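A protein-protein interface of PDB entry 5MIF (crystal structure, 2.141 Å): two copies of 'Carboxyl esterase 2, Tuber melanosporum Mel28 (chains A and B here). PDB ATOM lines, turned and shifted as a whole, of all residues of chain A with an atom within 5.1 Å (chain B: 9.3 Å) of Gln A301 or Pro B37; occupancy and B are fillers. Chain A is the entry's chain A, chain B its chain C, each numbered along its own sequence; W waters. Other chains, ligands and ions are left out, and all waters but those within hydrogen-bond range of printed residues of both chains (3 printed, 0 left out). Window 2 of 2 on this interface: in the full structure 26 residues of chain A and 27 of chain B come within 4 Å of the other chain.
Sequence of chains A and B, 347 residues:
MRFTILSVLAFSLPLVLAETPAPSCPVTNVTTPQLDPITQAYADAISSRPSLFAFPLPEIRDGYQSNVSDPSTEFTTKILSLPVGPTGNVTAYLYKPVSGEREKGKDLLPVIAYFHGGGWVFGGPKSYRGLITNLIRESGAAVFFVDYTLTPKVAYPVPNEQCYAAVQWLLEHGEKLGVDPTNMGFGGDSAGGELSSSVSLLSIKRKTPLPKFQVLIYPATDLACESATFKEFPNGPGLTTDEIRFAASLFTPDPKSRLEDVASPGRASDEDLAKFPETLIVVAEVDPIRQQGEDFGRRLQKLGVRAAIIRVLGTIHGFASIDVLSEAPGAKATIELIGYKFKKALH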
ATOM      1  N   GLY A 297      -6.156 -14.134   6.481  1.00  0.00           N
ATOM      2  CA  GLY A 297      -6.830 -12.850   6.426  1.00  0.00           C
ATOM      3  C   GLY A 297      -7.547 -12.599   5.104  1.00  0.00           C
ATOM      4  O   GLY A 297      -8.712 -12.186   5.101  1.00  0.00           O
ATOM      5  N   ARG A 298      -6.877 -12.889   3.989  1.00  0.00           N
ATOM      6  CA  ARG A 298      -7.487 -12.720   2.660  1.00  0.00           C
ATOM      7  C   ARG A 298      -8.734 -13.579   2.544  1.00  0.00           C
ATOM      8  O   ARG A 298      -9.748 -13.172   1.973  1.00  0.00           O
ATOM      9  CB  ARG A 298      -6.507 -13.087   1.548  1.00  0.00           C
ATOM     10  CG  ARG A 298      -5.327 -12.158   1.441  1.00  0.00           C
ATOM     11  CD  ARG A 298      -4.438 -12.567   0.291  1.00  0.00           C
ATOM     12  NE  ARG A 298      -3.396 -11.585   0.022  1.00  0.00           N
ATOM     13  CZ  ARG A 298      -2.094 -11.834   0.136  1.00  0.00           C
ATOM     14  NH1 ARG A 298      -1.676 -13.035   0.529  1.00  0.00           N
ATOM     15  NH2 ARG A 298      -1.207 -10.880  -0.138  1.00  0.00           N
ATOM     16  N   ARG A 299      -8.655 -14.773   3.117  1.00  0.00           N
ATOM     17  CA  ARG A 299      -9.788 -15.678   3.128  1.00  0.00           C
ATOM     18  C   ARG A 299     -10.965 -15.097   3.947  1.00  0.00           C
ATOM     19  O   ARG A 299     -12.108 -15.135   3.499  1.00  0.00           O
ATOM     20  CB  ARG A 299      -9.332 -17.034   3.653  1.00  0.00           C
ATOM     21  CG  ARG A 299     -10.394 -18.051   3.663  1.00  0.00           C
ATOM     22  CD  ARG A 299      -9.905 -19.407   3.217  1.00  0.00           C
ATOM     23  NE  ARG A 299     -11.089 -20.240   3.139  1.00  0.00           N
ATOM     24  CZ  ARG A 299     -11.301 -21.330   3.855  1.00  0.00           C
ATOM     25  NH1 ARG A 299     -10.361 -21.784   4.679  1.00  0.00           N
ATOM     26  NH2 ARG A 299     -12.447 -21.980   3.709  1.00  0.00           N
ATOM     27  N   LEU A 300     -10.685 -14.516   5.110  1.00  0.00           N
ATOM     28  CA  LEU A 300     -11.729 -13.843   5.892  1.00  0.00           C
ATOM     29  C   LEU A 300     -12.337 -12.668   5.120  1.00  0.00           C
ATOM     30  O   LEU A 300     -13.550 -12.439   5.160  1.00  0.00           O
ATOM     31  CB  LEU A 300     -11.169 -13.325   7.219  1.00  0.00           C
ATOM     32  CG  LEU A 300     -10.659 -14.354   8.218  1.00  0.00           C
ATOM     33  CD1 LEU A 300     -10.024 -13.654   9.405  1.00  0.00           C
ATOM     34  CD2 LEU A 300     -11.814 -15.225   8.671  1.00  0.00           C
ATOM     35  N   GLN A 301     -11.486 -11.921   4.424  1.00  0.00           N
ATOM     36  CA  GLN A 301     -11.941 -10.766   3.653  1.00  0.00           C
ATOM     37  C   GLN A 301     -12.925 -11.181   2.562  1.00  0.00           C
ATOM     38  O   GLN A 301     -14.022 -10.635   2.462  1.00  0.00           O
ATOM     39  CB  GLN A 301     -10.759 -10.037   3.031  1.00  0.00           C
ATOM     40  CG  GLN A 301     -10.031  -9.128   4.007  1.00  0.00           C
ATOM     41  CD  GLN A 301      -8.847  -8.429   3.376  1.00  0.00           C
ATOM     42  OE1 GLN A 301      -8.502  -8.682   2.217  1.00  0.00           O
ATOM     43  NE2 GLN A 301      -8.228  -7.522   4.128  1.00  0.00           N
ATOM     44  N   LYS A 302     -12.536 -12.185   1.786  1.00  0.00           N
ATOM     45  CA  LYS A 302     -13.362 -12.746   0.713  1.00  0.00           C
ATOM     46  C   LYS A 302     -14.718 -13.260   1.203  1.00  0.00           C
ATOM     47  O   LYS A 302     -15.711 -13.215   0.477  1.00  0.00           O
ATOM     48  CB  LYS A 302     -12.586 -13.878   0.041  1.00  0.00           C
ATOM     49  CG  LYS A 302     -13.397 -14.811  -0.833  1.00  0.00           C
ATOM     50  CD  LYS A 302     -12.484 -15.861  -1.456  1.00  0.00           C
ATOM     51  CE  LYS A 302     -13.230 -17.159  -1.747  1.00  0.00           C
ATOM     52  NZ  LYS A 302     -12.733 -17.811  -2.989  1.00  0.00           N
ATOM     53  N   LEU A 303     -14.772 -13.707   2.451  1.00  0.00           N
ATOM     54  CA  LEU A 303     -15.993 -14.297   2.993  1.00  0.00           C
ATOM     55  C   LEU A 303     -16.877 -13.286   3.683  1.00  0.00           C
ATOM     56  O   LEU A 303     -17.904 -13.634   4.260  1.00  0.00           O
ATOM     57  CB  LEU A 303     -15.646 -15.433   3.941  1.00  0.00           C
ATOM     58  CG  LEU A 303     -14.932 -16.561   3.209  1.00  0.00           C
ATOM     59  CD1 LEU A 303     -14.418 -17.611   4.181  1.00  0.00           C
ATOM     60  CD2 LEU A 303     -15.909 -17.182   2.208  1.00  0.00           C
ATOM     61  N   GLY A 304     -16.455 -12.029   3.656  1.00  0.00           N
ATOM     62  CA  GLY A 304     -17.274 -10.942   4.156  1.00  0.00           C
ATOM     63  C   GLY A 304     -17.083 -10.633   5.627  1.00  0.00           C
ATOM     64  O   GLY A 304     -17.858  -9.873   6.218  1.00  0.00           O
ATOM     65  N   VAL A 305     -16.047 -11.210   6.231  1.00  0.00           N
ATOM     66  CA  VAL A 305     -15.692 -10.846   7.604  1.00  0.00           C
ATOM     67  C   VAL A 305     -14.856  -9.567   7.592  1.00  0.00           C
ATOM     68  O   VAL A 305     -13.954  -9.416   6.760  1.00  0.00           O
ATOM     69  CB  VAL A 305     -14.917 -11.983   8.308  1.00  0.00           C
ATOM     70  CG1 VAL A 305     -14.493 -11.556   9.693  1.00  0.00           C
ATOM     71  CG2 VAL A 305     -15.775 -13.240   8.376  1.00  0.00           C
ATOM     72  N   ALA A 307     -11.916  -7.897   8.244  1.00  0.00           N
ATOM     73  CA  ALA A 307     -10.596  -8.352   8.628  1.00  0.00           C
ATOM     74  C   ALA A 307      -9.520  -7.423   8.090  1.00  0.00           C
ATOM     75  O   ALA A 307      -9.414  -7.210   6.878  1.00  0.00           O
ATOM     76  CB  ALA A 307     -10.355  -9.783   8.143  1.00  0.00           C
ATOM     77  N   ALA A 308      -8.721  -6.879   9.004  1.00  0.00           N
ATOM     78  CA  ALA A 308      -7.590  -6.040   8.643  1.00  0.00           C
ATOM     79  C   ALA A 308      -6.299  -6.851   8.733  1.00  0.00           C
ATOM     80  O   ALA A 308      -6.096  -7.611   9.682  1.00  0.00           O
ATOM     81  CB  ALA A 308      -7.530  -4.811   9.546  1.00  0.00           C
ATOM     82  N   ILE A 309      -5.432  -6.695   7.738  1.00  0.00           N
ATOM     83  CA  ILE A 309      -4.148  -7.392   7.719  1.00  0.00           C
ATOM     84  C   ILE A 309      -2.987  -6.419   7.522  1.00  0.00           C
ATOM     85  O   ILE A 309      -2.949  -5.640   6.562  1.00  0.00           O
ATOM     86  CB  ILE A 309      -4.072  -8.464   6.605  1.00  0.00           C
ATOM     87  CG1 ILE A 309      -5.384  -9.249   6.496  1.00  0.00           C
ATOM     88  CG2 ILE A 309      -2.882  -9.384   6.849  1.00  0.00           C
ATOM     89  CD1 ILE A 309      -5.680  -9.727   5.098  1.00  0.00           C
ATOM     90  N   GLN B  34      -7.947 -10.355  -3.787  1.00  0.00           N
ATOM     91  CA  GLN B  34      -6.732  -9.682  -3.352  1.00  0.00           C
ATOM     92  C   GLN B  34      -7.082  -8.380  -2.639  1.00  0.00           C
ATOM     93  O   GLN B  34      -6.418  -8.006  -1.679  1.00  0.00           O
ATOM     94  CB  GLN B  34      -5.800  -9.432  -4.526  1.00  0.00           C
ATOM     95  CG  GLN B  34      -4.345  -9.429  -4.106  1.00  0.00           C
ATOM     96  CD  GLN B  34      -3.405  -9.608  -5.277  1.00  0.00           C
ATOM     97  OE1 GLN B  34      -3.812  -9.496  -6.439  1.00  0.00           O
ATOM     98  NE2 GLN B  34      -2.140  -9.908  -4.981  1.00  0.00           N
ATOM     99  N   LEU B  35      -8.121  -7.698  -3.108  1.00  0.00           N
ATOM    100  CA  LEU B  35      -8.657  -6.519  -2.426  1.00  0.00           C
ATOM    101  C   LEU B  35      -9.825  -6.894  -1.517  1.00  0.00           C
ATOM    102  O   LEU B  35     -10.610  -7.774  -1.846  1.00  0.00           O
ATOM    103  CB  LEU B  35      -9.132  -5.459  -3.424  1.00  0.00           C
ATOM    104  CG  LEU B  35      -8.225  -4.429  -4.090  1.00  0.00           C
ATOM    105  CD1 LEU B  35      -6.860  -4.938  -4.443  1.00  0.00           C
ATOM    106  CD2 LEU B  35      -8.926  -3.882  -5.330  1.00  0.00           C
ATOM    107  N   ASP B  36      -9.946  -6.217  -0.379  1.00  0.00           N
ATOM    108  CA  ASP B  36     -11.100  -6.404   0.491  1.00  0.00           C
ATOM    109  C   ASP B  36     -12.357  -5.907  -0.236  1.00  0.00           C
ATOM    110  O   ASP B  36     -12.267  -5.063  -1.130  1.00  0.00           O
ATOM    111  CB  ASP B  36     -10.903  -5.666   1.822  1.00  0.00           C
ATOM    112  CG  ASP B  36     -11.063  -4.162   1.686  1.00  0.00           C
ATOM    113  OD1 ASP B  36     -12.211  -3.675   1.785  1.00  0.00           O
ATOM    114  OD2 ASP B  36     -10.042  -3.471   1.476  1.00  0.00           O
ATOM    115  N   PRO B  37     -13.530  -6.441   0.134  1.00  0.00           N
ATOM    116  CA  PRO B  37     -14.789  -6.148  -0.566  1.00  0.00           C
ATOM    117  C   PRO B  37     -15.103  -4.660  -0.740  1.00  0.00           C
ATOM    118  O   PRO B  37     -15.554  -4.259  -1.816  1.00  0.00           O
ATOM    119  CB  PRO B  37     -15.837  -6.805   0.331  1.00  0.00           C
ATOM    120  CG  PRO B  37     -15.114  -7.955   0.933  1.00  0.00           C
ATOM    121  CD  PRO B  37     -13.714  -7.467   1.178  1.00  0.00           C
ATOM    122  N   ILE B  38     -14.884  -3.862   0.299  1.00  0.00           N
ATOM    123  CA  ILE B  38     -15.186  -2.437   0.227  1.00  0.00           C
ATOM    124  C   ILE B  38     -14.274  -1.740  -0.780  1.00  0.00           C
ATOM    125  O   ILE B  38     -14.748  -0.970  -1.618  1.00  0.00           O
ATOM    126  CB  ILE B  38     -15.063  -1.761   1.597  1.00  0.00           C
ATOM    127  CG1 ILE B  38     -16.078  -2.351   2.570  1.00  0.00           C
ATOM    128  CG2 ILE B  38     -15.254  -0.253   1.475  1.00  0.00           C
ATOM    129  CD1 ILE B  38     -16.064  -1.672   3.939  1.00  0.00           C
ATOM    130  N   THR B  39     -12.980  -2.042  -0.730  1.00  0.00           N
ATOM    131  CA  THR B  39     -12.026  -1.447  -1.659  1.00  0.00           C
ATOM    132  C   THR B  39     -12.266  -1.930  -3.091  1.00  0.00           C
ATOM    133  O   THR B  39     -12.180  -1.143  -4.045  1.00  0.00           O
ATOM    134  CB  THR B  39     -10.573  -1.759  -1.248  1.00  0.00           C
ATOM    135  OG1 THR B  39     -10.318  -1.208   0.049  1.00  0.00           O
ATOM    136  CG2 THR B  39      -9.599  -1.165  -2.238  1.00  0.00           C
ATOM    137  N   GLN B  40     -12.567  -3.219  -3.242  1.00  0.00           N
ATOM    138  CA  GLN B  40     -12.868  -3.778  -4.557  1.00  0.00           C
ATOM    139  C   GLN B  40     -14.094  -3.117  -5.185  1.00  0.00           C
ATOM    140  O   GLN B  40     -14.085  -2.772  -6.367  1.00  0.00           O
ATOM    141  CB  GLN B  40     -13.098  -5.290  -4.468  1.00  0.00           C
ATOM    142  CG  GLN B  40     -13.329  -5.941  -5.814  1.00  0.00           C
ATOM    143  CD  GLN B  40     -12.128  -5.837  -6.725  1.00  0.00           C
ATOM    144  OE1 GLN B  40     -11.083  -6.442  -6.481  1.00  0.00           O
ATOM    145  NE2 GLN B  40     -12.260  -5.037  -7.771  1.00  0.00           N
ATOM    146  N   ALA B  41     -15.137  -2.936  -4.385  1.00  0.00           N
ATOM    147  CA  ALA B  41     -16.351  -2.278  -4.850  1.00  0.00           C
ATOM    148  C   ALA B  41     -16.047  -0.852  -5.307  1.00  0.00           C
ATOM    149  O   ALA B  41     -16.565  -0.403  -6.330  1.00  0.00           O
ATOM    150  CB  ALA B  41     -17.421  -2.278  -3.758  1.00  0.00           C
ATOM    151  N   TYR B  42     -15.200  -0.146  -4.561  1.00  0.00           N
ATOM    152  CA  TYR B  42     -14.790   1.196  -4.966  1.00  0.00           C
ATOM    153  C   TYR B  42     -14.057   1.164  -6.299  1.00  0.00           C
ATOM    154  O   TYR B  42     -14.324   1.981  -7.174  1.00  0.00           O
ATOM    155  CB  TYR B  42     -13.908   1.850  -3.899  1.00  0.00           C
ATOM    156  CG  TYR B  42     -13.307   3.177  -4.322  1.00  0.00           C
ATOM    157  CD1 TYR B  42     -13.994   4.382  -4.131  1.00  0.00           C
ATOM    158  CD2 TYR B  42     -12.053   3.227  -4.912  1.00  0.00           C
ATOM    159  CE1 TYR B  42     -13.436   5.595  -4.522  1.00  0.00           C
ATOM    160  CE2 TYR B  42     -11.487   4.434  -5.302  1.00  0.00           C
ATOM    161  CZ  TYR B  42     -12.179   5.609  -5.109  1.00  0.00           C
ATOM    162  OH  TYR B  42     -11.588   6.789  -5.509  1.00  0.00           O
ATOM    163  N   ALA B  43     -13.125   0.229  -6.443  1.00  0.00           N
ATOM    164  CA  ALA B  43     -12.363   0.095  -7.679  1.00  0.00           C
ATOM    165  C   ALA B  43     -13.267  -0.230  -8.875  1.00  0.00           C
ATOM    166  O   ALA B  43     -13.076   0.296  -9.973  1.00  0.00           O
ATOM    167  CB  ALA B  43     -11.285  -0.972  -7.522  1.00  0.00           C
ATOM    168  N   ASP B  44     -14.254  -1.094  -8.657  1.00  0.00           N
ATOM    169  CA  ASP B  44     -15.176  -1.458  -9.726  1.00  0.00           C
ATOM    170  C   ASP B  44     -16.043  -0.260 -10.134  1.00  0.00           C
ATOM    171  O   ASP B  44     -16.215   0.021 -11.317  1.00  0.00           O
ATOM    172  CB  ASP B  44     -16.053  -2.647  -9.308  1.00  0.00           C
ATOM    173  CG  ASP B  44     -15.274  -3.962  -9.258  1.00  0.00           C
ATOM    174  OD1 ASP B  44     -14.184  -4.046  -9.863  1.00  0.00           O
ATOM    175  OD2 ASP B  44     -15.766  -4.921  -8.628  1.00  0.00           O
ATOM    176  N   ALA B  45     -16.569   0.448  -9.139  1.00  0.00           N
ATOM    177  CA  ALA B  45     -17.465   1.581  -9.361  1.00  0.00           C
ATOM    178  C   ALA B  45     -16.824   2.709 -10.174  1.00  0.00           C
ATOM    179  O   ALA B  45     -17.529   3.535 -10.761  1.00  0.00           O
ATOM    180  CB  ALA B  45     -17.963   2.121  -8.019  1.00  0.00           C
ATOM    181  N   GLU B 285      -0.826  -2.087  -0.228  1.00  0.00           N
ATOM    182  CA  GLU B 285      -0.283  -3.281  -0.883  1.00  0.00           C
ATOM    183  C   GLU B 285      -0.379  -3.175  -2.406  1.00  0.00           C
ATOM    184  O   GLU B 285       0.594  -3.414  -3.122  1.00  0.00           O
ATOM    185  CB  GLU B 285      -1.018  -4.552  -0.410  1.00  0.00           C
ATOM    186  CG  GLU B 285      -0.558  -5.836  -1.120  1.00  0.00           C
ATOM    187  CD  GLU B 285      -1.421  -7.066  -0.799  1.00  0.00           C
ATOM    188  OE1 GLU B 285      -2.629  -6.925  -0.547  1.00  0.00           O
ATOM    189  OE2 GLU B 285      -0.885  -8.181  -0.813  1.00  0.00           O
ATOM    190  N   VAL B 286      -1.560  -2.819  -2.899  1.00  0.00           N
ATOM    191  CA  VAL B 286      -1.785  -2.792  -4.339  1.00  0.00           C
ATOM    192  C   VAL B 286      -1.621  -1.356  -4.845  1.00  0.00           C
ATOM    193  O   VAL B 286      -2.574  -0.583  -4.873  1.00  0.00           O
ATOM    194  CB  VAL B 286      -3.175  -3.358  -4.676  1.00  0.00           C
ATOM    195  CG1 VAL B 286      -3.412  -3.365  -6.180  1.00  0.00           C
ATOM    196  CG2 VAL B 286      -3.303  -4.777  -4.106  1.00  0.00           C
ATOM    197  N   VAL B 312      -0.263  -2.359   4.419  1.00  0.00           N
ATOM    198  CA  VAL B 312      -1.669  -2.703   4.636  1.00  0.00           C
ATOM    199  C   VAL B 312      -2.198  -3.536   3.471  1.00  0.00           C
ATOM    200  O   VAL B 312      -2.190  -3.085   2.325  1.00  0.00           O
ATOM    201  CB  VAL B 312      -2.543  -1.445   4.805  1.00  0.00           C
ATOM    202  CG1 VAL B 312      -3.948  -1.834   5.230  1.00  0.00           C
ATOM    203  CG2 VAL B 312      -1.910  -0.502   5.819  1.00  0.00           C
ATOM    204  N   LEU B 313      -2.634  -4.756   3.753  1.00  0.00           N
ATOM    205  CA  LEU B 313      -3.044  -5.672   2.685  1.00  0.00           C
ATOM    206  C   LEU B 313      -4.466  -5.429   2.185  1.00  0.00           C
ATOM    207  O   LEU B 313      -5.363  -5.056   2.950  1.00  0.00           O
ATOM    208  CB  LEU B 313      -2.917  -7.132   3.148  1.00  0.00           C
ATOM    209  CG  LEU B 313      -1.542  -7.786   2.957  1.00  0.00           C
ATOM    210  CD1 LEU B 313      -0.476  -7.105   3.814  1.00  0.00           C
ATOM    211  CD2 LEU B 313      -1.595  -9.294   3.243  1.00  0.00           C
ATOM    212  N   GLY B 314      -4.679  -5.690   0.901  1.00  0.00           N
ATOM    213  CA  GLY B 314      -6.018  -5.642   0.335  1.00  0.00           C
ATOM    214  C   GLY B 314      -6.544  -4.245   0.053  1.00  0.00           C
ATOM    215  O   GLY B 314      -7.736  -4.078  -0.225  1.00  0.00           O
ATOM    216  N   THR B 315      -5.672  -3.238   0.128  1.00  0.00           N
ATOM    217  CA  THR B 315      -6.104  -1.870  -0.134  1.00  0.00           C
ATOM    218  C   THR B 315      -5.218  -1.171  -1.168  1.00  0.00           C
ATOM    219  O   THR B 315      -4.198  -1.708  -1.591  1.00  0.00           O
ATOM    220  CB  THR B 315      -6.138  -1.027   1.146  1.00  0.00           C
ATOM    221  OG1 THR B 315      -6.824   0.206   0.870  1.00  0.00           O
ATOM    222  CG2 THR B 315      -4.718  -0.740   1.657  1.00  0.00           C
ATOM    223  N   VAL B 324     -14.735   6.678   1.199  1.00  0.00           N
ATOM    224  CA  VAL B 324     -15.196   5.294   1.092  1.00  0.00           C
ATOM    225  C   VAL B 324     -14.090   4.296   1.467  1.00  0.00           C
ATOM    226  O   VAL B 324     -14.310   3.385   2.241  1.00  0.00           O
ATOM    227  CB  VAL B 324     -15.716   4.991  -0.331  1.00  0.00           C
ATOM    228  CG1 VAL B 324     -15.765   3.500  -0.587  1.00  0.00           C
ATOM    229  CG2 VAL B 324     -17.090   5.608  -0.532  1.00  0.00           C
ATOM    230  N   LEU B 325     -12.891   4.488   0.934  1.00  0.00           N
ATOM    231  CA  LEU B 325     -11.793   3.573   1.213  1.00  0.00           C
ATOM    232  C   LEU B 325     -11.369   3.588   2.670  1.00  0.00           C
ATOM    233  O   LEU B 325     -10.935   2.563   3.219  1.00  0.00           O
ATOM    234  CB  LEU B 325     -10.593   3.917   0.357  1.00  0.00           C
ATOM    235  CG  LEU B 325     -10.791   3.666  -1.126  1.00  0.00           C
ATOM    236  CD1 LEU B 325      -9.491   3.992  -1.864  1.00  0.00           C
ATOM    237  CD2 LEU B 325     -11.198   2.213  -1.319  1.00  0.00           C
ATOM    238  N   ALA B 328     -12.855   0.994   5.256  1.00  0.00           N
ATOM    239  CA  ALA B 328     -12.463  -0.413   5.208  1.00  0.00           C
ATOM    240  C   ALA B 328     -11.566  -0.742   6.415  1.00  0.00           C
ATOM    241  O   ALA B 328     -10.899   0.149   6.930  1.00  0.00           O
ATOM    242  CB  ALA B 328     -11.745  -0.713   3.896  1.00  0.00           C
ATOM    243  N   PRO B 329     -11.565  -2.008   6.880  1.00  0.00           N
ATOM    244  CA  PRO B 329     -10.893  -2.347   8.155  1.00  0.00           C
ATOM    245  C   PRO B 329      -9.414  -1.928   8.237  1.00  0.00           C
ATOM    246  O   PRO B 329      -9.038  -1.219   9.174  1.00  0.00           O
ATOM    247  CB  PRO B 329     -11.032  -3.879   8.237  1.00  0.00           C
ATOM    248  CG  PRO B 329     -12.271  -4.197   7.438  1.00  0.00           C
ATOM    249  CD  PRO B 329     -12.350  -3.137   6.340  1.00  0.00           C
ATOM    250  N   GLY B 330      -8.603  -2.350   7.270  1.00  0.00           N
ATOM    251  CA  GLY B 330      -7.183  -2.033   7.252  1.00  0.00           C
ATOM    252  C   GLY B 330      -6.886  -0.543   7.184  1.00  0.00           C
ATOM    253  O   GLY B 330      -6.044  -0.039   7.911  1.00  0.00           O
ATOM    254  N   ALA B 331      -7.582   0.166   6.302  1.00  0.00           N
ATOM    255  CA  ALA B 331      -7.422   1.609   6.187  1.00  0.00           C
ATOM    256  C   ALA B 331      -7.766   2.290   7.498  1.00  0.00           C
ATOM    257  O   ALA B 331      -7.038   3.159   7.976  1.00  0.00           O
ATOM    258  CB  ALA B 331      -8.307   2.161   5.069  1.00  0.00           C
HETATM  259  O   HOH W   1      -9.034  -4.658   5.231  1.00  0.00           O
HETATM  260  O   HOH W   2      -3.899  -9.171  -0.498  1.00  0.00           O
HETATM  261  O   HOH W   3      -6.089  -4.815   5.669  1.00  0.00           O
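The guanidinium group (NH2) of Arg A298 is in salt-bridge range of the side-chain carboxylate (OE2) of Glu B285. The backbone carbonyl oxygen of Ile A309 sits at hydrogen-bond distance from the backbone NH of Leu B313, at 3.0 Å.
NE2 of Gln A301 is in hydrogen-bond range of O of Ala A307. The backbone NH (N) of Ile B38 sits at hydrogen-bond distance from the side-chain carboxylate (OD1) of Asp B36. The side-chain carboxylate of Asp B36 sits at hydrogen-bond distance from the side-chain hydroxyl of Thr B39 (2.7 Å). O of Gly B314 is in hydrogen-bond range of N of Asp B36. The backbone carbonyl oxygen (O) of Val B312 lies within hydrogen-bond range of the backbone NH (N) of Glu B285, at 3.1 Å. The side-chain carboxylate of Glu B285 sits at hydrogen-bond distance from the backbone NH of Gly B314.
NH2 of Arg A298 touches CD2 of Leu B313 (3.8 Å). CD of Gln A301 touches CB of Asp B36 (3.8 Å). Gln A301 touches Pro B37 (O to CG, 3.3 Å). Leu B313 touches Gln A301. Pro B329 touches Ala A307. Ala A308 touches Pro B329. CB of Ala A308 touches N of Gly B330, 3.5 Å away. Val B312 touches Ile A309 (CA to O, 3.7 Å).
Of chain B, only Asp B36 (3.8 Å), Pro B37 (3.3 Å) and Leu B313 (3.96 Å) come within 4 Å of Gln A301. Pro B37 touches one residue of chain A. Thr B39 touches none of the printed residues of chain A. Ala B41 touches none of the printed residues of chain A. Of the printed residues of chain A, Val B312 touches Ile A309 (3.7 Å). Of the printed residues of chain A, Pro B329 touches Ala A307 and Ala A308. The nearest printed residue of chain A that does not touch Asp B36 is Ala A307 (5.5 Å).
Of the 24 printed residues of chain B, 7 touch a printed residue of chain A. Of the 12 printed residues of chain A, 5 touch a printed residue of chain B. Hydrophobic or aromatic side chains of chain A that line the printed part of chain B: Ala A308 and Ile A309. Among the printed residues, 10 pairs touch across the chains. Among the printed residues, Asp or Glu carboxylates within 4 Å of a Lys or Arg side-chain nitrogen of the other chain: Arg A298 with Glu B285.
No position is printed for both chains.
Water W2 lies within hydrogen-bond range of the guanidinium group (NE) of Arg A298 (2.5 Å), the side-chain carboxylate (OE1) of Glu B285 (2.6 Å) and the backbone carbonyl oxygen (O) of Gln B34 (3.0 Å). Water W3 bridges O of Leu B313 (2.8 Å) and N of Ile A309 (2.9 Å). Water W1 lies within hydrogen-bond range of O of Ala A307 (3.1 Å), N of Gly B330 (3.1 Å) and NE2 of Gln A301 (3.2 Å).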
